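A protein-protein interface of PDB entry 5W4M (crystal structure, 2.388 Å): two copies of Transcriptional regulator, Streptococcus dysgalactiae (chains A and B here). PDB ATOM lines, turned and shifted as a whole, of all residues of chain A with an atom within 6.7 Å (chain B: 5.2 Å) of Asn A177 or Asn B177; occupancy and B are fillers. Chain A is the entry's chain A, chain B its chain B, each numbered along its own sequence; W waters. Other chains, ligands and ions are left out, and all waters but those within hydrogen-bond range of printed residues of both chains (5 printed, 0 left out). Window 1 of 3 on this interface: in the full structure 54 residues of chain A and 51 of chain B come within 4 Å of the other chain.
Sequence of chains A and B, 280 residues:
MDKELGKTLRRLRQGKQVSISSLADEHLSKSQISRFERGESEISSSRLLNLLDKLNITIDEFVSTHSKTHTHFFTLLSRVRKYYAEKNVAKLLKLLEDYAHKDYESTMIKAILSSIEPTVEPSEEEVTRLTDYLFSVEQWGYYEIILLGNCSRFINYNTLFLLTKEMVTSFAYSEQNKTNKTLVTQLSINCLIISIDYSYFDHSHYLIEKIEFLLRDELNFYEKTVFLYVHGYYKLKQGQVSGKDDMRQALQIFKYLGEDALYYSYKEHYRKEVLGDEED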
ATOM      1  N   THR A  58      -5.828  12.018  39.126  1.00  0.00           N
ATOM      2  CA  THR A  58      -6.533  11.806  37.871  1.00  0.00           C
ATOM      3  C   THR A  58      -7.732  10.896  38.103  1.00  0.00           C
ATOM      4  O   THR A  58      -7.726  10.035  38.987  1.00  0.00           O
ATOM      5  CB  THR A  58      -5.630  11.171  36.805  1.00  0.00           C
ATOM      6  OG1 THR A  58      -5.615   9.751  36.974  1.00  0.00           O
ATOM      7  CG2 THR A  58      -4.221  11.655  36.905  1.00  0.00           C
ATOM      8  N   ASP A  60      -8.361   8.717  36.032  1.00  0.00           N
ATOM      9  CA  ASP A  60      -7.810   7.432  35.615  1.00  0.00           C
ATOM     10  C   ASP A  60      -7.057   6.758  36.754  1.00  0.00           C
ATOM     11  O   ASP A  60      -7.129   5.533  36.913  1.00  0.00           O
ATOM     12  CB  ASP A  60      -6.898   7.617  34.403  1.00  0.00           C
ATOM     13  CG  ASP A  60      -6.352   6.303  33.879  1.00  0.00           C
ATOM     14  OD1 ASP A  60      -5.176   5.991  34.161  1.00  0.00           O
ATOM     15  OD2 ASP A  60      -7.106   5.574  33.200  1.00  0.00           O
ATOM     16  N   GLU A  61      -6.325   7.539  37.556  1.00  0.00           N
ATOM     17  CA  GLU A  61      -5.676   6.977  38.736  1.00  0.00           C
ATOM     18  C   GLU A  61      -6.707   6.458  39.729  1.00  0.00           C
ATOM     19  O   GLU A  61      -6.496   5.422  40.368  1.00  0.00           O
ATOM     20  CB  GLU A  61      -4.780   8.023  39.403  1.00  0.00           C
ATOM     21  CG  GLU A  61      -3.415   8.205  38.752  1.00  0.00           C
ATOM     22  CD  GLU A  61      -2.708   9.472  39.216  1.00  0.00           C
ATOM     23  OE1 GLU A  61      -3.384  10.372  39.762  1.00  0.00           O
ATOM     24  OE2 GLU A  61      -1.475   9.567  39.041  1.00  0.00           O
ATOM     25  N   ALA A 172     -10.253   8.679  20.211  1.00  0.00           N
ATOM     26  CA  ALA A 172     -10.326   9.434  21.456  1.00  0.00           C
ATOM     27  C   ALA A 172      -8.979   9.357  22.162  1.00  0.00           C
ATOM     28  O   ALA A 172      -8.591   8.295  22.661  1.00  0.00           O
ATOM     29  CB  ALA A 172     -11.441   8.895  22.348  1.00  0.00           C
ATOM     30  N   TYR A 173      -8.267  10.478  22.207  1.00  0.00           N
ATOM     31  CA  TYR A 173      -7.037  10.565  22.977  1.00  0.00           C
ATOM     32  C   TYR A 173      -7.000  11.903  23.698  1.00  0.00           C
ATOM     33  O   TYR A 173      -7.533  12.905  23.214  1.00  0.00           O
ATOM     34  CB  TYR A 173      -5.792  10.377  22.091  1.00  0.00           C
ATOM     35  CG  TYR A 173      -5.123  11.656  21.636  1.00  0.00           C
ATOM     36  CD1 TYR A 173      -4.049  12.192  22.337  1.00  0.00           C
ATOM     37  CD2 TYR A 173      -5.555  12.320  20.494  1.00  0.00           C
ATOM     38  CE1 TYR A 173      -3.433  13.356  21.921  1.00  0.00           C
ATOM     39  CE2 TYR A 173      -4.943  13.483  20.069  1.00  0.00           C
ATOM     40  CZ  TYR A 173      -3.884  13.997  20.786  1.00  0.00           C
ATOM     41  OH  TYR A 173      -3.272  15.156  20.368  1.00  0.00           O
ATOM     42  N   SER A 174      -6.381  11.898  24.872  1.00  0.00           N
ATOM     43  CA  SER A 174      -6.208  13.090  25.681  1.00  0.00           C
ATOM     44  C   SER A 174      -4.745  13.508  25.673  1.00  0.00           C
ATOM     45  O   SER A 174      -3.846  12.680  25.483  1.00  0.00           O
ATOM     46  CB  SER A 174      -6.670  12.851  27.122  1.00  0.00           C
ATOM     47  OG  SER A 174      -5.716  12.085  27.837  1.00  0.00           O
ATOM     48  N   GLU A 175      -4.513  14.802  25.886  1.00  0.00           N
ATOM     49  CA  GLU A 175      -3.149  15.305  25.964  1.00  0.00           C
ATOM     50  C   GLU A 175      -2.401  14.766  27.177  1.00  0.00           C
ATOM     51  O   GLU A 175      -1.169  14.854  27.215  1.00  0.00           O
ATOM     52  CB  GLU A 175      -3.160  16.835  25.979  1.00  0.00           C
ATOM     53  CG  GLU A 175      -1.940  17.470  25.323  1.00  0.00           C
ATOM     54  CD  GLU A 175      -1.746  17.025  23.881  1.00  0.00           C
ATOM     55  OE1 GLU A 175      -2.745  16.944  23.133  1.00  0.00           O
ATOM     56  OE2 GLU A 175      -0.587  16.748  23.498  1.00  0.00           O
ATOM     57  N   GLN A 176      -3.109  14.191  28.149  1.00  0.00           N
ATOM     58  CA  GLN A 176      -2.483  13.638  29.339  1.00  0.00           C
ATOM     59  C   GLN A 176      -2.342  12.123  29.304  1.00  0.00           C
ATOM     60  O   GLN A 176      -1.458  11.585  29.979  1.00  0.00           O
ATOM     61  CB  GLN A 176      -3.275  14.039  30.588  1.00  0.00           C
ATOM     62  CG  GLN A 176      -2.446  14.027  31.851  1.00  0.00           C
ATOM     63  CD  GLN A 176      -3.289  14.133  33.098  1.00  0.00           C
ATOM     64  OE1 GLN A 176      -4.310  14.826  33.122  1.00  0.00           O
ATOM     65  NE2 GLN A 176      -2.875  13.430  34.143  1.00  0.00           N
ATOM     66  N   ASN A 177      -3.184  11.424  28.545  1.00  0.00           N
ATOM     67  CA  ASN A 177      -3.097   9.972  28.393  1.00  0.00           C
ATOM     68  C   ASN A 177      -3.030   9.654  26.901  1.00  0.00           C
ATOM     69  O   ASN A 177      -4.060   9.613  26.221  1.00  0.00           O
ATOM     70  CB  ASN A 177      -4.275   9.271  29.061  1.00  0.00           C
ATOM     71  CG  ASN A 177      -4.181   7.758  28.972  1.00  0.00           C
ATOM     72  OD1 ASN A 177      -3.146   7.209  28.587  1.00  0.00           O
ATOM     73  ND2 ASN A 177      -5.268   7.076  29.321  1.00  0.00           N
ATOM     74  N   LYS A 178      -1.815   9.422  26.403  1.00  0.00           N
ATOM     75  CA  LYS A 178      -1.570   9.140  24.995  1.00  0.00           C
ATOM     76  C   LYS A 178      -1.666   7.652  24.660  1.00  0.00           C
ATOM     77  O   LYS A 178      -1.153   7.232  23.615  1.00  0.00           O
ATOM     78  CB  LYS A 178      -0.192   9.669  24.588  1.00  0.00           C
ATOM     79  CG  LYS A 178       0.033  11.148  24.873  1.00  0.00           C
ATOM     80  CD  LYS A 178      -0.451  12.015  23.721  1.00  0.00           C
ATOM     81  CE  LYS A 178      -0.104  13.484  23.942  1.00  0.00           C
ATOM     82  NZ  LYS A 178       1.361  13.709  24.084  1.00  0.00           N
ATOM     83  N   THR A 179      -2.307   6.853  25.519  1.00  0.00           N
ATOM     84  CA  THR A 179      -2.346   5.406  25.310  1.00  0.00           C
ATOM     85  C   THR A 179      -2.997   5.053  23.979  1.00  0.00           C
ATOM     86  O   THR A 179      -2.434   4.295  23.181  1.00  0.00           O
ATOM     87  CB  THR A 179      -3.084   4.723  26.465  1.00  0.00           C
ATOM     88  OG1 THR A 179      -2.347   4.902  27.680  1.00  0.00           O
ATOM     89  CG2 THR A 179      -3.243   3.238  26.195  1.00  0.00           C
ATOM     90  N   ASN A 180      -4.189   5.597  23.717  1.00  0.00           N
ATOM     91  CA  ASN A 180      -4.872   5.286  22.466  1.00  0.00           C
ATOM     92  C   ASN A 180      -4.093   5.814  21.267  1.00  0.00           C
ATOM     93  O   ASN A 180      -4.024   5.149  20.226  1.00  0.00           O
ATOM     94  CB  ASN A 180      -6.289   5.859  22.480  1.00  0.00           C
ATOM     95  CG  ASN A 180      -7.184   5.190  23.512  1.00  0.00           C
ATOM     96  OD1 ASN A 180      -6.862   4.124  24.038  1.00  0.00           O
ATOM     97  ND2 ASN A 180      -8.317   5.820  23.805  1.00  0.00           N
ATOM     98  N   LYS A 181      -3.498   7.005  21.395  1.00  0.00           N
ATOM     99  CA  LYS A 181      -2.740   7.577  20.285  1.00  0.00           C
ATOM    100  C   LYS A 181      -1.576   6.676  19.889  1.00  0.00           C
ATOM    101  O   LYS A 181      -1.284   6.510  18.699  1.00  0.00           O
ATOM    102  CB  LYS A 181      -2.239   8.976  20.650  1.00  0.00           C
ATOM    103  CG  LYS A 181      -1.484   9.676  19.521  1.00  0.00           C
ATOM    104  CD  LYS A 181      -1.036  11.078  19.921  1.00  0.00           C
ATOM    105  CE  LYS A 181      -0.353  11.789  18.762  1.00  0.00           C
ATOM    106  NZ  LYS A 181       0.087  13.167  19.119  1.00  0.00           N
ATOM    107  N   ASP B  60     -11.828   7.666  31.298  1.00  0.00           N
ATOM    108  CA  ASP B  60     -10.863   8.640  30.801  1.00  0.00           C
ATOM    109  C   ASP B  60     -11.255   9.164  29.422  1.00  0.00           C
ATOM    110  O   ASP B  60     -11.170  10.370  29.165  1.00  0.00           O
ATOM    111  CB  ASP B  60      -9.470   8.014  30.770  1.00  0.00           C
ATOM    112  CG  ASP B  60      -8.367   9.047  30.791  1.00  0.00           C
ATOM    113  OD1 ASP B  60      -8.374   9.901  31.701  1.00  0.00           O
ATOM    114  OD2 ASP B  60      -7.489   8.998  29.903  1.00  0.00           O
ATOM    115  N   SER B 174      -0.562   0.935  37.171  1.00  0.00           N
ATOM    116  CA  SER B 174      -1.704   0.797  36.275  1.00  0.00           C
ATOM    117  C   SER B 174      -1.343  -0.154  35.144  1.00  0.00           C
ATOM    118  O   SER B 174      -0.336   0.046  34.454  1.00  0.00           O
ATOM    119  CB  SER B 174      -2.137   2.150  35.705  1.00  0.00           C
ATOM    120  OG  SER B 174      -3.246   1.997  34.834  1.00  0.00           O
ATOM    121  N   GLU B 175      -2.170  -1.183  34.954  1.00  0.00           N
ATOM    122  CA  GLU B 175      -1.909  -2.161  33.903  1.00  0.00           C
ATOM    123  C   GLU B 175      -2.183  -1.591  32.518  1.00  0.00           C
ATOM    124  O   GLU B 175      -1.554  -2.011  31.541  1.00  0.00           O
ATOM    125  CB  GLU B 175      -2.757  -3.413  34.139  1.00  0.00           C
ATOM    126  CG  GLU B 175      -2.093  -4.720  33.733  1.00  0.00           C
ATOM    127  CD  GLU B 175      -2.792  -5.931  34.327  1.00  0.00           C
ATOM    128  OE1 GLU B 175      -3.308  -6.768  33.554  1.00  0.00           O
ATOM    129  OE2 GLU B 175      -2.830  -6.041  35.572  1.00  0.00           O
ATOM    130  N   GLN B 176      -3.103  -0.631  32.414  1.00  0.00           N
ATOM    131  CA  GLN B 176      -3.564  -0.138  31.124  1.00  0.00           C
ATOM    132  C   GLN B 176      -2.985   1.216  30.740  1.00  0.00           C
ATOM    133  O   GLN B 176      -2.987   1.556  29.552  1.00  0.00           O
ATOM    134  CB  GLN B 176      -5.094  -0.045  31.116  1.00  0.00           C
ATOM    135  CG  GLN B 176      -5.728  -0.317  29.765  1.00  0.00           C
ATOM    136  CD  GLN B 176      -7.104   0.309  29.628  1.00  0.00           C
ATOM    137  OE1 GLN B 176      -7.332   1.145  28.752  1.00  0.00           O
ATOM    138  NE2 GLN B 176      -8.030  -0.095  30.495  1.00  0.00           N
ATOM    139  N   ASN B 177      -2.496   1.994  31.703  1.00  0.00           N
ATOM    140  CA  ASN B 177      -1.987   3.342  31.452  1.00  0.00           C
ATOM    141  C   ASN B 177      -0.568   3.422  32.006  1.00  0.00           C
ATOM    142  O   ASN B 177      -0.375   3.567  33.218  1.00  0.00           O
ATOM    143  CB  ASN B 177      -2.900   4.394  32.080  1.00  0.00           C
ATOM    144  CG  ASN B 177      -2.472   5.815  31.755  1.00  0.00           C
ATOM    145  OD1 ASN B 177      -1.483   6.038  31.054  1.00  0.00           O
ATOM    146  ND2 ASN B 177      -3.228   6.789  32.258  1.00  0.00           N
ATOM    147  N   LYS B 178       0.420   3.346  31.117  1.00  0.00           N
ATOM    148  CA  LYS B 178       1.826   3.320  31.499  1.00  0.00           C
ATOM    149  C   LYS B 178       2.421   4.710  31.685  1.00  0.00           C
ATOM    150  O   LYS B 178       3.639   4.825  31.853  1.00  0.00           O
ATOM    151  CB  LYS B 178       2.642   2.553  30.455  1.00  0.00           C
ATOM    152  CG  LYS B 178       2.107   1.167  30.149  1.00  0.00           C
ATOM    153  CD  LYS B 178       2.388   0.212  31.290  1.00  0.00           C
ATOM    154  CE  LYS B 178       2.003  -1.206  30.917  1.00  0.00           C
ATOM    155  NZ  LYS B 178       2.533  -2.165  31.916  1.00  0.00           N
ATOM    156  N   THR B 179       1.593   5.757  31.671  1.00  0.00           N
ATOM    157  CA  THR B 179       2.106   7.123  31.727  1.00  0.00           C
ATOM    158  C   THR B 179       2.953   7.354  32.973  1.00  0.00           C
ATOM    159  O   THR B 179       4.073   7.867  32.887  1.00  0.00           O
ATOM    160  CB  THR B 179       0.947   8.121  31.675  1.00  0.00           C
ATOM    161  OG1 THR B 179       0.222   7.950  30.451  1.00  0.00           O
ATOM    162  CG2 THR B 179       1.464   9.552  31.754  1.00  0.00           C
ATOM    163  N   ASN B 180       2.438   6.975  34.146  1.00  0.00           N
ATOM    164  CA  ASN B 180       3.178   7.231  35.381  1.00  0.00           C
ATOM    165  C   ASN B 180       4.429   6.362  35.474  1.00  0.00           C
ATOM    166  O   ASN B 180       5.485   6.829  35.919  1.00  0.00           O
ATOM    167  CB  ASN B 180       2.274   7.015  36.597  1.00  0.00           C
ATOM    168  CG  ASN B 180       1.228   8.116  36.760  1.00  0.00           C
ATOM    169  OD1 ASN B 180       1.250   9.127  36.057  1.00  0.00           O
ATOM    170  ND2 ASN B 180       0.311   7.922  37.704  1.00  0.00           N
HETATM  171  O   HOH W   1      -0.421   3.126  28.162  1.00  0.00           O
HETATM  172  O   HOH W   2      -7.005   3.848  26.985  1.00  0.00           O
HETATM  173  O   HOH W   3      -9.977   5.337  32.475  1.00  0.00           O
HETATM  174  O   HOH W   4      -2.086   9.482  32.069  1.00  0.00           O
HETATM  175  O   HOH W   5      -7.412  10.753  33.988  1.00  0.00           O
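OD1 of Asp A60 sits at hydrogen-bond distance from ND2 of Asn B177, at 2.8 Å.
The side-chain amide nitrogen (ND2) of Asn B180 lies within hydrogen-bond range of the side-chain carboxylate (OE2) of Glu A61 (2.8 Å).
The side-chain carboxylate (OD2) of Asp B60 is in hydrogen-bond range of the side-chain amide nitrogen (ND2) of Asn A177, at 3.0 Å.
The side-chain amide oxygen (OD1) of Asn A177 lies close to the side-chain amide oxygen (OD1) of Asn B177, at 3.2 Å.
The side-chain hydroxyl (OG1) of Thr A58 lies close to the backbone NH (N) of Asp A60, at 3.1 Å.
The side-chain hydroxyl (OG) of Ser A174 sits close to the backbone NH (N) of Gln A176, 3.4 Å away.
OG of Ser A174 is in hydrogen-bond range of N of Asn A177, at 2.7 Å.
OD1 of Asn A177 lies within hydrogen-bond range of OG1 of Thr A179, 2.6 Å away.
The side-chain hydroxyl (OG) of Ser B174 sits at hydrogen-bond distance from the backbone NH (N) of Asn B177, 3.2 Å away.
The side-chain hydroxyl of Thr B179 sits at hydrogen-bond distance from the side-chain amide oxygen of Asn B177 (2.6 Å).
CB of Asp A60 touches OD1 of Asp B60, at 3.8 Å.
Gln A176 touches Thr B179.
Thr B179 touches Asn A177 (OG1 to OD1, 3.9 Å).
Thr A179 touches Gln B176 (CG2 to O, 3.8 Å).
Thr A179 touches Asn B177.
Of chain B, only Asp B60, Asn B177 and Thr B179 come within 4 Å of Asn A177.
Of the printed residues of chain A, Asn B177 touches Asp A60, Asn A177 and Thr A179.
Of the printed residues of chain A, Gln B176 touches Thr A179 (3.8 Å).
Printed residues of chain B within 4 Å of Gln A176: Thr B179 (3.98 Å).
Of the 8 printed residues of chain B, 5 touch a printed residue of chain A.
Printed residues of chain B that touch a printed residue of chain A: Asp B60, Gln B176, Asn B177, Thr B179 and Asn B180.
Asp B60 touches its own counterpart, Asp A60.
Asp A60 touches Asn B177, and with the chains exchanged Asn A177 touches Asp B60.
Gln A176 touches Thr B179, and with the chains exchanged Thr A179 touches Gln B176.
Asn A177 touches its own counterpart, Asn B177.
Of the 9 pairs that touch across the chains among the printed residues, 8 have their exchanged pair printed and touching as well.
Water W5 lies within hydrogen-bond range of the side-chain carboxylate (OD1) of Asp B60 (2.6 Å) and the backbone NH (N) of Asp A60 (3.0 Å).
Water W1 lies within hydrogen-bond range of OG1 of Thr A179 (2.7 Å), N of Lys B178 (3.1 Å) and O of Gln B176 (3.3 Å).
Water W4 lies within hydrogen-bond range of ND2 of Asn B177 (2.9 Å), O of Gln A176 (3.0 Å) and OG1 of Thr B179 (3.2 Å).
Water W2 lies within hydrogen-bond range of the side-chain amide oxygen of Asn A180 (3.0 Å) and the side-chain amide oxygen of Gln B176 (3.2 Å).
Water W3 bridges the side-chain carboxylate (OD2) of Asp A60 (3.0 Å) and the backbone NH (N) of Asp B60 (3.2 Å).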
